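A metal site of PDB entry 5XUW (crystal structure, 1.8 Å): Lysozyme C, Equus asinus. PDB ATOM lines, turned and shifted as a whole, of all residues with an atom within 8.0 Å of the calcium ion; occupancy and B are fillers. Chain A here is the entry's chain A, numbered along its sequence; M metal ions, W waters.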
ATOM      1  N   THR A  40      14.108 -16.226  -2.070  1.00  0.00           N
ATOM      2  CA  THR A  40      15.178 -15.668  -1.235  1.00  0.00           C
ATOM      3  C   THR A  40      15.036 -16.027   0.227  1.00  0.00           C
ATOM      4  O   THR A  40      16.003 -15.927   0.967  1.00  0.00           O
ATOM      5  CB  THR A  40      15.246 -14.124  -1.326  1.00  0.00           C
ATOM      6  OG1 THR A  40      14.002 -13.568  -0.893  1.00  0.00           O
ATOM      7  CG2 THR A  40      15.545 -13.671  -2.737  1.00  0.00           C
ATOM      8  N   GLY A  55      18.681 -19.116   1.998  1.00  0.00           N
ATOM      9  CA  GLY A  55      18.444 -18.210   0.894  1.00  0.00           C
ATOM     10  C   GLY A  55      18.384 -18.842  -0.474  1.00  0.00           C
ATOM     11  O   GLY A  55      18.313 -20.064  -0.611  1.00  0.00           O
ATOM     12  N   LEU A  56      18.420 -17.968  -1.476  1.00  0.00           N
ATOM     13  CA  LEU A  56      18.303 -18.323  -2.892  1.00  0.00           C
ATOM     14  C   LEU A  56      19.320 -19.379  -3.344  1.00  0.00           C
ATOM     15  O   LEU A  56      18.988 -20.245  -4.155  1.00  0.00           O
ATOM     16  CB  LEU A  56      18.475 -17.070  -3.749  1.00  0.00           C
ATOM     17  CG  LEU A  56      18.240 -17.137  -5.252  1.00  0.00           C
ATOM     18  CD1 LEU A  56      16.788 -17.445  -5.560  1.00  0.00           C
ATOM     19  CD2 LEU A  56      18.635 -15.820  -5.900  1.00  0.00           C
ATOM     20  N   ILE A  78      29.694 -12.776   6.681  1.00  0.00           N
ATOM     21  CA  ILE A  78      28.332 -12.291   6.624  1.00  0.00           C
ATOM     22  C   ILE A  78      27.393 -13.055   7.561  1.00  0.00           C
ATOM     23  O   ILE A  78      27.520 -14.271   7.733  1.00  0.00           O
ATOM     24  CB  ILE A  78      27.829 -12.317   5.155  1.00  0.00           C
ATOM     25  CG1 ILE A  78      26.583 -11.445   4.985  1.00  0.00           C
ATOM     26  CG2 ILE A  78      27.591 -13.741   4.667  1.00  0.00           C
ATOM     27  CD1 ILE A  78      26.197 -11.250   3.533  1.00  0.00           C
ATOM     28  N   MET A  79      26.462 -12.315   8.158  1.00  0.00           N
ATOM     29  CA  MET A  79      25.404 -12.898   8.961  1.00  0.00           C
ATOM     30  C   MET A  79      24.445 -13.649   8.053  1.00  0.00           C
ATOM     31  O   MET A  79      24.062 -13.125   7.003  1.00  0.00           O
ATOM     32  CB  MET A  79      24.630 -11.812   9.730  1.00  0.00           C
ATOM     33  CG  MET A  79      24.490 -12.088  11.210  1.00  0.00           C
ATOM     34  SD  MET A  79      26.088 -12.017  12.015  1.00  0.00           S
ATOM     35  CE  MET A  79      25.658 -12.609  13.648  1.00  0.00           C
ATOM     36  N   CYS A  80      24.031 -14.852   8.459  1.00  0.00           N
ATOM     37  CA  CYS A  80      23.162 -15.675   7.610  1.00  0.00           C
ATOM     38  C   CYS A  80      21.806 -15.016   7.320  1.00  0.00           C
ATOM     39  O   CYS A  80      21.239 -15.237   6.248  1.00  0.00           O
ATOM     40  CB  CYS A  80      22.939 -17.060   8.204  1.00  0.00           C
ATOM     41  SG  CYS A  80      24.407 -18.119   8.337  1.00  0.00           S
ATOM     42  N   SER A  81      21.323 -14.189   8.246  1.00  0.00           N
ATOM     43  CA  SER A  81      20.062 -13.445   8.049  1.00  0.00           C
ATOM     44  C   SER A  81      20.060 -12.523   6.821  1.00  0.00           C
ATOM     45  O   SER A  81      19.002 -12.282   6.236  1.00  0.00           O
ATOM     46  CB  SER A  81      19.736 -12.621   9.303  1.00  0.00           C
ATOM     47  OG  SER A  81      20.799 -11.755   9.637  1.00  0.00           O
ATOM     48  N   LYS A  82      21.240 -12.043   6.431  1.00  0.00           N
ATOM     49  CA  LYS A  82      21.379 -11.193   5.247  1.00  0.00           C
ATOM     50  C   LYS A  82      21.228 -11.958   3.929  1.00  0.00           C
ATOM     51  O   LYS A  82      21.224 -11.362   2.855  1.00  0.00           O
ATOM     52  CB  LYS A  82      22.701 -10.450   5.276  1.00  0.00           C
ATOM     53  CG  LYS A  82      22.845  -9.571   6.526  1.00  0.00           C
ATOM     54  CD  LYS A  82      24.280  -9.166   6.777  1.00  0.00           C
ATOM     55  CE  LYS A  82      24.723  -8.045   5.866  1.00  0.00           C
ATOM     56  NZ  LYS A  82      24.140  -6.736   6.299  1.00  0.00           N
ATOM     57  N   LEU A  83      21.133 -13.282   4.021  1.00  0.00           N
ATOM     58  CA  LEU A  83      20.824 -14.124   2.868  1.00  0.00           C
ATOM     59  C   LEU A  83      19.335 -14.477   2.797  1.00  0.00           C
ATOM     60  O   LEU A  83      18.955 -15.365   2.047  1.00  0.00           O
ATOM     61  CB  LEU A  83      21.687 -15.396   2.938  1.00  0.00           C
ATOM     62  CG  LEU A  83      23.182 -15.146   3.110  1.00  0.00           C
ATOM     63  CD1 LEU A  83      23.917 -16.447   3.367  1.00  0.00           C
ATOM     64  CD2 LEU A  83      23.747 -14.416   1.905  1.00  0.00           C
ATOM     65  N   LEU A  84      18.506 -13.815   3.611  1.00  0.00           N
ATOM     66  CA  LEU A  84      17.062 -14.051   3.610  1.00  0.00           C
ATOM     67  C   LEU A  84      16.247 -12.825   3.209  1.00  0.00           C
ATOM     68  O   LEU A  84      15.035 -12.896   3.175  1.00  0.00           O
ATOM     69  CB  LEU A  84      16.613 -14.577   4.976  1.00  0.00           C
ATOM     70  CG  LEU A  84      17.175 -15.926   5.430  1.00  0.00           C
ATOM     71  CD1 LEU A  84      16.699 -16.222   6.843  1.00  0.00           C
ATOM     72  CD2 LEU A  84      16.774 -17.042   4.485  1.00  0.00           C
ATOM     73  N   ASP A  85      16.909 -11.708   2.910  1.00  0.00           N
ATOM     74  CA  ASP A  85      16.198 -10.479   2.509  1.00  0.00           C
ATOM     75  C   ASP A  85      15.965 -10.488   0.997  1.00  0.00           C
ATOM     76  O   ASP A  85      16.291 -11.466   0.309  1.00  0.00           O
ATOM     77  CB  ASP A  85      16.951  -9.231   2.972  1.00  0.00           C
ATOM     78  CG  ASP A  85      18.272  -9.047   2.283  1.00  0.00           C
ATOM     79  OD1 ASP A  85      18.875 -10.064   1.928  1.00  0.00           O
ATOM     80  OD2 ASP A  85      18.708  -7.887   2.106  1.00  0.00           O
ATOM     81  N   ASP A  86      15.392  -9.413   0.454  1.00  0.00           N
ATOM     82  CA  ASP A  86      15.004  -9.393  -0.956  1.00  0.00           C
ATOM     83  C   ASP A  86      16.187  -9.180  -1.889  1.00  0.00           C
ATOM     84  O   ASP A  86      16.150  -9.648  -3.026  1.00  0.00           O
ATOM     85  CB  ASP A  86      13.953  -8.306  -1.230  1.00  0.00           C
ATOM     86  CG  ASP A  86      12.583  -8.657  -0.711  1.00  0.00           C
ATOM     87  OD1 ASP A  86      12.409  -9.711  -0.065  1.00  0.00           O
ATOM     88  OD2 ASP A  86      11.639  -7.884  -0.975  1.00  0.00           O
ATOM     89  N   ASN A  87      17.209  -8.450  -1.426  1.00  0.00           N
ATOM     90  CA  ASN A  87      18.330  -8.092  -2.288  1.00  0.00           C
ATOM     91  C   ASN A  87      19.376  -9.185  -2.241  1.00  0.00           C
ATOM     92  O   ASN A  87      19.743  -9.622  -1.169  1.00  0.00           O
ATOM     93  CB  ASN A  87      18.920  -6.758  -1.864  1.00  0.00           C
ATOM     94  CG  ASN A  87      19.856  -6.214  -2.921  1.00  0.00           C
ATOM     95  OD1 ASN A  87      19.428  -5.594  -3.900  1.00  0.00           O
ATOM     96  ND2 ASN A  87      21.133  -6.446  -2.738  1.00  0.00           N
ATOM     97  N   ILE A  88      19.860  -9.619  -3.408  1.00  0.00           N
ATOM     98  CA  ILE A  88      20.747 -10.791  -3.474  1.00  0.00           C
ATOM     99  C   ILE A  88      22.194 -10.463  -3.848  1.00  0.00           C
ATOM    100  O   ILE A  88      22.976 -11.360  -4.137  1.00  0.00           O
ATOM    101  CB  ILE A  88      20.198 -11.893  -4.416  1.00  0.00           C
ATOM    102  CG1 ILE A  88      20.110 -11.420  -5.870  1.00  0.00           C
ATOM    103  CG2 ILE A  88      18.843 -12.373  -3.927  1.00  0.00           C
ATOM    104  CD1 ILE A  88      19.968 -12.552  -6.870  1.00  0.00           C
ATOM    105  N   ASP A  89      22.562  -9.189  -3.851  1.00  0.00           N
ATOM    106  CA  ASP A  89      23.934  -8.807  -4.159  1.00  0.00           C
ATOM    107  C   ASP A  89      24.949  -9.480  -3.246  1.00  0.00           C
ATOM    108  O   ASP A  89      25.972  -9.977  -3.736  1.00  0.00           O
ATOM    109  CB  ASP A  89      24.123  -7.281  -4.110  1.00  0.00           C
ATOM    110  CG  ASP A  89      23.426  -6.574  -5.265  1.00  0.00           C
ATOM    111  OD1 ASP A  89      22.906  -7.249  -6.175  1.00  0.00           O
ATOM    112  OD2 ASP A  89      23.380  -5.318  -5.242  1.00  0.00           O
ATOM    113  N   ASP A  90      24.674  -9.515  -1.935  1.00  0.00           N
ATOM    114  CA  ASP A  90      25.594 -10.171  -1.005  1.00  0.00           C
ATOM    115  C   ASP A  90      25.536 -11.697  -1.131  1.00  0.00           C
ATOM    116  O   ASP A  90      26.573 -12.378  -1.006  1.00  0.00           O
ATOM    117  CB  ASP A  90      25.439  -9.681   0.450  1.00  0.00           C
ATOM    118  CG  ASP A  90      24.010  -9.724   0.965  1.00  0.00           C
ATOM    119  OD1 ASP A  90      23.147 -10.363   0.332  1.00  0.00           O
ATOM    120  OD2 ASP A  90      23.756  -9.093   2.019  1.00  0.00           O
ATOM    121  N   ASP A  91      24.361 -12.233  -1.456  1.00  0.00           N
ATOM    122  CA  ASP A  91      24.233 -13.667  -1.808  1.00  0.00           C
ATOM    123  C   ASP A  91      25.104 -14.011  -3.011  1.00  0.00           C
ATOM    124  O   ASP A  91      25.793 -15.046  -3.032  1.00  0.00           O
ATOM    125  CB  ASP A  91      22.794 -14.075  -2.133  1.00  0.00           C
ATOM    126  CG  ASP A  91      21.816 -13.765  -1.018  1.00  0.00           C
ATOM    127  OD1 ASP A  91      21.635 -12.565  -0.718  1.00  0.00           O
ATOM    128  OD2 ASP A  91      21.195 -14.704  -0.480  1.00  0.00           O
ATOM    129  N   ILE A  92      25.065 -13.140  -4.018  1.00  0.00           N
ATOM    130  CA  ILE A  92      25.848 -13.346  -5.243  1.00  0.00           C
ATOM    131  C   ILE A  92      27.347 -13.277  -4.958  1.00  0.00           C
ATOM    132  O   ILE A  92      28.126 -14.116  -5.424  1.00  0.00           O
ATOM    133  CB  ILE A  92      25.473 -12.307  -6.326  1.00  0.00           C
ATOM    134  CG1 ILE A  92      24.075 -12.623  -6.900  1.00  0.00           C
ATOM    135  CG2 ILE A  92      26.507 -12.257  -7.450  1.00  0.00           C
ATOM    136  CD1 ILE A  92      23.448 -11.477  -7.653  1.00  0.00           C
HETATM  137 CA    CA M   1      20.757 -10.735   0.677  1.00  0.00          CA
HETATM  138  O   HOH W   1      21.184  -8.489   1.232  1.00  0.00           O
HETATM  139  O   HOH W   2      18.990 -12.316   0.233  1.00  0.00           O
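ND2 of Asn 87 lies close to N of Asp 89 (3.3 Å).
The backbone carbonyl oxygen (O) of Asp 85 lies close to the side-chain hydroxyl (OG1) of Thr 40.
Along chain A the residues within 4 Å of the calcium ion span positions 82 to 91.
The calcium ion is bound by O of Lys 82 (2.3 Å), water W1 (2.4 Å), OD1 of Asp 85 (2.4 Å), O of Asn 87 (2.4 Å), water W2 (2.4 Å), OD1 of Asp 90 (2.4 Å) and OD1 of Asp 91 (2.5 Å).
Water W2 lies within hydrogen-bond range of O of Asp 85 (2.8 Å) and OD2 of Asp 91 (3.3 Å).
Water W1 lies within hydrogen-bond range of OD2 of Asp 85 (2.7 Å) and OD2 of Asp 90 (2.8 Å).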
